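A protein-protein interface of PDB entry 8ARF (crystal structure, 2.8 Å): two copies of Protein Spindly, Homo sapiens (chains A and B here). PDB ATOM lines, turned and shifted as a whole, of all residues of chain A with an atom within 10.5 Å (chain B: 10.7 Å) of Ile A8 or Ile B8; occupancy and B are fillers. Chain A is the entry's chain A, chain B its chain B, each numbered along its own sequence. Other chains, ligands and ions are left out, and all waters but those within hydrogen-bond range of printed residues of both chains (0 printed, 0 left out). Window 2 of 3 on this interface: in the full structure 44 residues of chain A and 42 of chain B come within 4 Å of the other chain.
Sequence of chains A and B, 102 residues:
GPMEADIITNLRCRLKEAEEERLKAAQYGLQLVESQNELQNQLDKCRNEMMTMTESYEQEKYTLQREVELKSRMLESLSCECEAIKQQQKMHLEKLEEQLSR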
ATOM      1  N   GLU A   4      19.821 -30.510 -11.128  1.00  0.00           N
ATOM      2  CA  GLU A   4      18.734 -29.787 -11.875  1.00  0.00           C
ATOM      3  C   GLU A   4      17.565 -30.680 -12.313  1.00  0.00           C
ATOM      4  O   GLU A   4      17.244 -30.715 -13.475  1.00  0.00           O
ATOM      5  CB  GLU A   4      19.291 -28.973 -13.052  1.00  0.00           C
ATOM      6  CG  GLU A   4      20.048 -27.727 -12.588  1.00  0.00           C
ATOM      7  CD  GLU A   4      21.049 -27.162 -13.607  1.00  0.00           C
ATOM      8  OE1 GLU A   4      20.991 -27.547 -14.800  1.00  0.00           O
ATOM      9  OE2 GLU A   4      21.900 -26.334 -13.189  1.00  0.00           O
ATOM     10  N   ALA A   5      17.031 -31.455 -11.356  1.00  0.00           N
ATOM     11  CA  ALA A   5      15.613 -31.798 -11.250  1.00  0.00           C
ATOM     12  C   ALA A   5      15.046 -30.847 -10.186  1.00  0.00           C
ATOM     13  O   ALA A   5      14.006 -31.135  -9.612  1.00  0.00           O
ATOM     14  CB  ALA A   5      15.384 -33.264 -10.844  1.00  0.00           C
ATOM     15  N   ASP A   6      15.699 -29.696  -9.987  1.00  0.00           N
ATOM     16  CA  ASP A   6      15.207 -28.645  -9.121  1.00  0.00           C
ATOM     17  C   ASP A   6      14.613 -27.564 -10.041  1.00  0.00           C
ATOM     18  O   ASP A   6      13.463 -27.150  -9.859  1.00  0.00           O
ATOM     19  CB  ASP A   6      16.309 -28.080  -8.237  1.00  0.00           C
ATOM     20  CG  ASP A   6      17.266 -29.155  -7.702  1.00  0.00           C
ATOM     21  OD1 ASP A   6      17.029 -29.670  -6.608  1.00  0.00           O
ATOM     22  OD2 ASP A   6      18.297 -29.454  -8.323  1.00  0.00           O
ATOM     23  N   ILE A   7      15.395 -27.126 -11.039  1.00  0.00           N
ATOM     24  CA  ILE A   7      14.934 -26.118 -11.980  1.00  0.00           C
ATOM     25  C   ILE A   7      13.888 -26.713 -12.930  1.00  0.00           C
ATOM     26  O   ILE A   7      12.909 -26.021 -13.271  1.00  0.00           O
ATOM     27  CB  ILE A   7      16.077 -25.400 -12.747  1.00  0.00           C
ATOM     28  CG1 ILE A   7      16.630 -26.267 -13.898  1.00  0.00           C
ATOM     29  CG2 ILE A   7      17.161 -24.958 -11.768  1.00  0.00           C
ATOM     30  CD1 ILE A   7      16.579 -25.572 -15.242  1.00  0.00           C
ATOM     31  N   ILE A   8      14.076 -27.988 -13.319  1.00  0.00           N
ATOM     32  CA  ILE A   8      13.169 -28.627 -14.259  1.00  0.00           C
ATOM     33  C   ILE A   8      11.819 -28.767 -13.589  1.00  0.00           C
ATOM     34  O   ILE A   8      10.801 -28.370 -14.205  1.00  0.00           O
ATOM     35  CB  ILE A   8      13.707 -29.979 -14.806  1.00  0.00           C
ATOM     36  CG1 ILE A   8      14.967 -29.768 -15.693  1.00  0.00           C
ATOM     37  CG2 ILE A   8      12.590 -30.779 -15.526  1.00  0.00           C
ATOM     38  CD1 ILE A   8      14.852 -28.885 -16.903  1.00  0.00           C
ATOM     39  N   THR A   9      11.821 -29.317 -12.359  1.00  0.00           N
ATOM     40  CA  THR A   9      10.597 -29.470 -11.568  1.00  0.00           C
ATOM     41  C   THR A   9       9.716 -28.215 -11.676  1.00  0.00           C
ATOM     42  O   THR A   9       8.509 -28.296 -11.995  1.00  0.00           O
ATOM     43  CB  THR A   9      10.921 -29.752 -10.074  1.00  0.00           C
ATOM     44  OG1 THR A   9      11.281 -31.120  -9.942  1.00  0.00           O
ATOM     45  CG2 THR A   9       9.725 -29.458  -9.095  1.00  0.00           C
ATOM     46  N   ASN A  10      10.334 -27.059 -11.397  1.00  0.00           N
ATOM     47  CA  ASN A  10       9.617 -25.791 -11.365  1.00  0.00           C
ATOM     48  C   ASN A  10       9.134 -25.444 -12.788  1.00  0.00           C
ATOM     49  O   ASN A  10       7.934 -25.278 -12.998  1.00  0.00           O
ATOM     50  CB  ASN A  10      10.444 -24.670 -10.669  1.00  0.00           C
ATOM     51  CG  ASN A  10      11.247 -23.821 -11.638  1.00  0.00           C
ATOM     52  OD1 ASN A  10      10.687 -23.129 -12.481  1.00  0.00           O
ATOM     53  ND2 ASN A  10      12.561 -23.855 -11.512  1.00  0.00           N
ATOM     54  N   LEU A  11      10.068 -25.388 -13.751  1.00  0.00           N
ATOM     55  CA  LEU A  11       9.755 -25.003 -15.145  1.00  0.00           C
ATOM     56  C   LEU A  11       8.605 -25.836 -15.752  1.00  0.00           C
ATOM     57  O   LEU A  11       7.787 -25.334 -16.489  1.00  0.00           O
ATOM     58  CB  LEU A  11      10.990 -25.075 -16.050  1.00  0.00           C
ATOM     59  CG  LEU A  11      11.531 -23.675 -16.404  1.00  0.00           C
ATOM     60  CD1 LEU A  11      12.372 -23.170 -15.250  1.00  0.00           C
ATOM     61  CD2 LEU A  11      12.311 -23.601 -17.701  1.00  0.00           C
ATOM     62  N   ARG A  12       8.536 -27.115 -15.380  1.00  0.00           N
ATOM     63  CA  ARG A  12       7.472 -27.992 -15.822  1.00  0.00           C
ATOM     64  C   ARG A  12       6.206 -27.411 -15.237  1.00  0.00           C
ATOM     65  O   ARG A  12       5.286 -27.072 -16.010  1.00  0.00           O
ATOM     66  CB  ARG A  12       7.735 -29.485 -15.457  1.00  0.00           C
ATOM     67  CG  ARG A  12       8.461 -30.200 -16.585  1.00  0.00           C
ATOM     68  CD  ARG A  12       8.920 -31.651 -16.380  1.00  0.00           C
ATOM     69  NE  ARG A  12       9.469 -32.142 -17.671  1.00  0.00           N
ATOM     70  CZ  ARG A  12      10.391 -33.100 -17.874  1.00  0.00           C
ATOM     71  NH1 ARG A  12      10.936 -33.787 -16.873  1.00  0.00           N
ATOM     72  NH2 ARG A  12      10.748 -33.385 -19.130  1.00  0.00           N
ATOM     73  N   CYS A  13       6.167 -27.269 -13.899  1.00  0.00           N
ATOM     74  CA  CYS A  13       4.998 -26.719 -13.188  1.00  0.00           C
ATOM     75  C   CYS A  13       4.604 -25.310 -13.703  1.00  0.00           C
ATOM     76  O   CYS A  13       3.429 -24.984 -13.677  1.00  0.00           O
ATOM     77  CB  CYS A  13       5.212 -26.697 -11.657  1.00  0.00           C
ATOM     78  SG  CYS A  13       5.296 -25.040 -10.897  1.00  0.00           S
ATOM     79  N   ARG A  14       5.592 -24.507 -14.129  1.00  0.00           N
ATOM     80  CA  ARG A  14       5.348 -23.184 -14.693  1.00  0.00           C
ATOM     81  C   ARG A  14       4.600 -23.256 -16.034  1.00  0.00           C
ATOM     82  O   ARG A  14       3.582 -22.572 -16.222  1.00  0.00           O
ATOM     83  CB  ARG A  14       6.631 -22.377 -14.846  1.00  0.00           C
ATOM     84  CG  ARG A  14       6.383 -20.880 -15.091  1.00  0.00           C
ATOM     85  CD  ARG A  14       5.320 -20.240 -14.169  1.00  0.00           C
ATOM     86  NE  ARG A  14       4.749 -18.982 -14.691  1.00  0.00           N
ATOM     87  CZ  ARG A  14       4.217 -18.008 -13.939  1.00  0.00           C
ATOM     88  NH1 ARG A  14       4.178 -18.088 -12.604  1.00  0.00           N
ATOM     89  NH2 ARG A  14       3.713 -16.921 -14.514  1.00  0.00           N
ATOM     90  N   LEU A  15       5.112 -24.066 -16.966  1.00  0.00           N
ATOM     91  CA  LEU A  15       4.380 -24.349 -18.182  1.00  0.00           C
ATOM     92  C   LEU A  15       2.978 -24.878 -17.858  1.00  0.00           C
ATOM     93  O   LEU A  15       2.023 -24.363 -18.350  1.00  0.00           O
ATOM     94  CB  LEU A  15       5.122 -25.354 -19.032  1.00  0.00           C
ATOM     95  CG  LEU A  15       5.704 -24.957 -20.371  1.00  0.00           C
ATOM     96  CD1 LEU A  15       6.072 -26.258 -21.070  1.00  0.00           C
ATOM     97  CD2 LEU A  15       4.768 -24.261 -21.317  1.00  0.00           C
ATOM     98  N   LYS A  16       2.864 -25.907 -17.024  1.00  0.00           N
ATOM     99  CA  LYS A  16       1.581 -26.487 -16.697  1.00  0.00           C
ATOM    100  C   LYS A  16       0.623 -25.354 -16.287  1.00  0.00           C
ATOM    101  O   LYS A  16      -0.506 -25.299 -16.745  1.00  0.00           O
ATOM    102  CB  LYS A  16       1.728 -27.556 -15.621  1.00  0.00           C
ATOM    103  CG  LYS A  16       0.451 -28.323 -15.188  1.00  0.00           C
ATOM    104  CD  LYS A  16       0.511 -29.004 -13.784  1.00  0.00           C
ATOM    105  CE  LYS A  16       0.855 -28.101 -12.569  1.00  0.00           C
ATOM    106  NZ  LYS A  16       1.454 -28.868 -11.439  1.00  0.00           N
ATOM    107  N   GLU B   4      20.398 -33.355 -21.050  1.00  0.00           N
ATOM    108  CA  GLU B   4      19.614 -32.884 -19.855  1.00  0.00           C
ATOM    109  C   GLU B   4      19.586 -31.353 -19.750  1.00  0.00           C
ATOM    110  O   GLU B   4      18.691 -30.798 -19.159  1.00  0.00           O
ATOM    111  CB  GLU B   4      20.169 -33.493 -18.560  1.00  0.00           C
ATOM    112  CG  GLU B   4      21.653 -33.195 -18.275  1.00  0.00           C
ATOM    113  CD  GLU B   4      22.658 -34.166 -18.931  1.00  0.00           C
ATOM    114  OE1 GLU B   4      23.207 -33.890 -20.026  1.00  0.00           O
ATOM    115  OE2 GLU B   4      22.915 -35.218 -18.327  1.00  0.00           O
ATOM    116  N   ALA B   5      20.559 -30.661 -20.341  1.00  0.00           N
ATOM    117  CA  ALA B   5      20.499 -29.218 -20.471  1.00  0.00           C
ATOM    118  C   ALA B   5      19.810 -28.855 -21.786  1.00  0.00           C
ATOM    119  O   ALA B   5      19.382 -27.733 -21.989  1.00  0.00           O
ATOM    120  CB  ALA B   5      21.885 -28.590 -20.414  1.00  0.00           C
ATOM    121  N   ASP B   6      19.742 -29.810 -22.713  1.00  0.00           N
ATOM    122  CA  ASP B   6      18.955 -29.631 -23.941  1.00  0.00           C
ATOM    123  C   ASP B   6      17.451 -29.730 -23.606  1.00  0.00           C
ATOM    124  O   ASP B   6      16.649 -29.159 -24.337  1.00  0.00           O
ATOM    125  CB  ASP B   6      19.371 -30.611 -25.041  1.00  0.00           C
ATOM    126  CG  ASP B   6      19.908 -31.899 -24.471  1.00  0.00           C
ATOM    127  OD1 ASP B   6      21.160 -32.038 -24.337  1.00  0.00           O
ATOM    128  OD2 ASP B   6      19.065 -32.752 -24.092  1.00  0.00           O
ATOM    129  N   ILE B   7      17.110 -30.436 -22.514  1.00  0.00           N
ATOM    130  CA  ILE B   7      15.754 -30.405 -21.963  1.00  0.00           C
ATOM    131  C   ILE B   7      15.381 -28.946 -21.615  1.00  0.00           C
ATOM    132  O   ILE B   7      14.355 -28.437 -22.036  1.00  0.00           O
ATOM    133  CB  ILE B   7      15.568 -31.279 -20.691  1.00  0.00           C
ATOM    134  CG1 ILE B   7      15.743 -32.760 -20.981  1.00  0.00           C
ATOM    135  CG2 ILE B   7      14.214 -31.086 -19.993  1.00  0.00           C
ATOM    136  CD1 ILE B   7      15.349 -33.656 -19.797  1.00  0.00           C
ATOM    137  N   ILE B   8      16.243 -28.261 -20.860  1.00  0.00           N
ATOM    138  CA  ILE B   8      15.925 -26.939 -20.350  1.00  0.00           C
ATOM    139  C   ILE B   8      15.703 -25.940 -21.495  1.00  0.00           C
ATOM    140  O   ILE B   8      14.832 -25.105 -21.413  1.00  0.00           O
ATOM    141  CB  ILE B   8      16.941 -26.422 -19.283  1.00  0.00           C
ATOM    142  CG1 ILE B   8      18.037 -25.508 -19.906  1.00  0.00           C
ATOM    143  CG2 ILE B   8      17.529 -27.604 -18.510  1.00  0.00           C
ATOM    144  CD1 ILE B   8      18.707 -24.571 -18.923  1.00  0.00           C
ATOM    145  N   THR B   9      16.470 -26.024 -22.578  1.00  0.00           N
ATOM    146  CA  THR B   9      16.304 -25.038 -23.642  1.00  0.00           C
ATOM    147  C   THR B   9      14.987 -25.233 -24.391  1.00  0.00           C
ATOM    148  O   THR B   9      14.345 -24.258 -24.743  1.00  0.00           O
ATOM    149  CB  THR B   9      17.525 -24.940 -24.589  1.00  0.00           C
ATOM    150  OG1 THR B   9      17.254 -23.950 -25.577  1.00  0.00           O
ATOM    151  CG2 THR B   9      17.843 -26.261 -25.274  1.00  0.00           C
ATOM    152  N   ASN B  10      14.566 -26.484 -24.571  1.00  0.00           N
ATOM    153  CA  ASN B  10      13.227 -26.779 -25.119  1.00  0.00           C
ATOM    154  C   ASN B  10      12.152 -26.181 -24.229  1.00  0.00           C
ATOM    155  O   ASN B  10      11.320 -25.468 -24.692  1.00  0.00           O
ATOM    156  CB  ASN B  10      12.943 -28.294 -25.282  1.00  0.00           C
ATOM    157  CG  ASN B  10      13.928 -28.969 -26.187  1.00  0.00           C
ATOM    158  OD1 ASN B  10      14.429 -28.355 -27.123  1.00  0.00           O
ATOM    159  ND2 ASN B  10      14.240 -30.212 -25.896  1.00  0.00           N
ATOM    160  N   LEU B  11      12.220 -26.482 -22.932  1.00  0.00           N
ATOM    161  CA  LEU B  11      11.257 -26.012 -21.957  1.00  0.00           C
ATOM    162  C   LEU B  11      11.231 -24.501 -21.867  1.00  0.00           C
ATOM    163  O   LEU B  11      10.192 -23.911 -21.781  1.00  0.00           O
ATOM    164  CB  LEU B  11      11.540 -26.580 -20.593  1.00  0.00           C
ATOM    165  CG  LEU B  11      11.246 -28.057 -20.284  1.00  0.00           C
ATOM    166  CD1 LEU B  11      10.701 -28.163 -18.845  1.00  0.00           C
ATOM    167  CD2 LEU B  11      10.297 -28.775 -21.261  1.00  0.00           C
ATOM    168  N   ARG B  12      12.386 -23.859 -21.948  1.00  0.00           N
ATOM    169  CA  ARG B  12      12.452 -22.400 -21.892  1.00  0.00           C
ATOM    170  C   ARG B  12      11.839 -21.813 -23.143  1.00  0.00           C
ATOM    171  O   ARG B  12      11.065 -20.860 -23.079  1.00  0.00           O
ATOM    172  CB  ARG B  12      13.892 -21.902 -21.748  1.00  0.00           C
ATOM    173  CG  ARG B  12      14.319 -21.611 -20.314  1.00  0.00           C
ATOM    174  CD  ARG B  12      15.804 -21.872 -20.129  1.00  0.00           C
ATOM    175  NE  ARG B  12      16.433 -20.963 -19.160  1.00  0.00           N
ATOM    176  CZ  ARG B  12      16.591 -21.190 -17.850  1.00  0.00           C
ATOM    177  NH1 ARG B  12      16.171 -22.312 -17.278  1.00  0.00           N
ATOM    178  NH2 ARG B  12      17.184 -20.276 -17.091  1.00  0.00           N
ATOM    179  N   CYS B  13      12.202 -22.366 -24.298  1.00  0.00           N
ATOM    180  CA  CYS B  13      11.573 -21.977 -25.551  1.00  0.00           C
ATOM    181  C   CYS B  13      10.064 -22.163 -25.441  1.00  0.00           C
ATOM    182  O   CYS B  13       9.315 -21.337 -25.910  1.00  0.00           O
ATOM    183  CB  CYS B  13      12.125 -22.794 -26.723  1.00  0.00           C
ATOM    184  SG  CYS B  13      10.973 -23.067 -28.085  1.00  0.00           S
ATOM    185  N   ARG B  14       9.642 -23.271 -24.840  1.00  0.00           N
ATOM    186  CA  ARG B  14       8.221 -23.603 -24.781  1.00  0.00           C
ATOM    187  C   ARG B  14       7.472 -22.647 -23.821  1.00  0.00           C
ATOM    188  O   ARG B  14       6.418 -22.150 -24.158  1.00  0.00           O
ATOM    189  CB  ARG B  14       7.974 -25.062 -24.378  1.00  0.00           C
ATOM    190  CG  ARG B  14       8.036 -26.073 -25.498  1.00  0.00           C
ATOM    191  CD  ARG B  14       6.687 -26.542 -25.946  1.00  0.00           C
ATOM    192  NE  ARG B  14       5.962 -27.326 -24.930  1.00  0.00           N
ATOM    193  CZ  ARG B  14       4.748 -27.003 -24.423  1.00  0.00           C
ATOM    194  NH1 ARG B  14       4.102 -25.868 -24.793  1.00  0.00           N
ATOM    195  NH2 ARG B  14       4.146 -27.819 -23.539  1.00  0.00           N
ATOM    196  N   LEU B  15       8.036 -22.403 -22.638  1.00  0.00           N
ATOM    197  CA  LEU B  15       7.493 -21.448 -21.689  1.00  0.00           C
ATOM    198  C   LEU B  15       7.245 -20.069 -22.335  1.00  0.00           C
ATOM    199  O   LEU B  15       6.182 -19.530 -22.227  1.00  0.00           O
ATOM    200  CB  LEU B  15       8.427 -21.264 -20.498  1.00  0.00           C
ATOM    201  CG  LEU B  15       7.822 -21.344 -19.092  1.00  0.00           C
ATOM    202  CD1 LEU B  15       8.501 -20.343 -18.170  1.00  0.00           C
ATOM    203  CD2 LEU B  15       6.316 -21.138 -19.077  1.00  0.00           C
ATOM    204  N   LYS B  16       8.243 -19.521 -23.025  1.00  0.00           N
ATOM    205  CA  LYS B  16       8.080 -18.291 -23.770  1.00  0.00           C
ATOM    206  C   LYS B  16       6.813 -18.325 -24.590  1.00  0.00           C
ATOM    207  O   LYS B  16       5.977 -17.412 -24.450  1.00  0.00           O
ATOM    208  CB  LYS B  16       9.293 -17.977 -24.685  1.00  0.00           C
ATOM    209  CG  LYS B  16      10.392 -17.171 -24.008  1.00  0.00           C
ATOM    210  CD  LYS B  16       9.831 -15.973 -23.211  1.00  0.00           C
ATOM    211  CE  LYS B  16      10.404 -15.837 -21.787  1.00  0.00           C
ATOM    212  NZ  LYS B  16      10.105 -16.996 -20.880  1.00  0.00           N
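O of Ile A7 is in hydrogen-bond range of ND2 of Asn A10, at 2.8 Å.
Among the printed residues, pairs that only touch across the chains: Ile A8 with Ile B8 (3.4 Å), Leu A15 with Arg B14 (3.5 Å), Arg A14 with Leu B15 (3.8 Å), Arg A12 with Leu B11 (3.8 Å), Leu A15 with Leu B15 (3.8 Å), Ile A8 with Ile B7 (3.8 Å), Leu A11 with Arg B12 (3.8 Å), Ile A7 with Arg B12 (3.9 Å) and Ile A7 with Ile B8 (3.96 Å).
No residue of chain B comes within 4 Å of Thr A9. No residue of chain B comes within 4 Å of Asn A10. Of chain B, only Arg B12 (3.8 Å) comes within 4 Å of Leu A11. Printed residues of chain B within 4 Å of Arg A14: Leu B15. Printed residues of chain B within 4 Å of Leu A15: Arg B14 and Leu B15. No residue of chain A comes within 4 Å of Ala B5. Of chain A, only Ile A8 (3.8 Å) comes within 4 Å of Ile B7. Ile B8 touches just these residues of chain A: Ile A7 (3.96 Å) and Ile A8 (3.4 Å). Thr B9 touches none of the printed residues of chain A. No residue of chain A comes within 4 Å of Asn B10. Of chain A, only Arg A12 comes within 4 Å of Leu B11. Arg B12 touches two residues of chain A. Of the printed residues of chain A, Arg B14 touches Leu A15 (3.5 Å). Printed residues of chain A within 4 Å of Leu B15: Arg A14 (3.8 Å) and Leu A15 (3.8 Å). Lys B16 touches none of the printed residues of chain A. The nearest residue of chain B that does not touch Ile A8 is Leu B11 (4.6 Å).
Of the 13 printed residues of chain A, 6 touch a printed residue of chain B. Hydrophobic or aromatic side chains of chain A that line the printed part of chain B: Ile A7, Ile A8, Leu A11 and Leu A15. Of the 13 printed residues of chain B, 6 touch a printed residue of chain A. Among the printed residues, 9 pairs touch across the chains. Among the printed residues, no Asp or Glu carboxylate lies within 4 Å of a Lys or Arg side-chain nitrogen of the other chain.
Ile A7 touches Ile B8, and with the chains exchanged Ile A8 touches Ile B7. Ile A7 touches Arg B12, but with the chains exchanged Arg A12 does not touch Ile B7 (4.2 Å). Ile A8 touches its own counterpart, Ile B8. Leu A15 touches its own counterpart, Leu B15.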
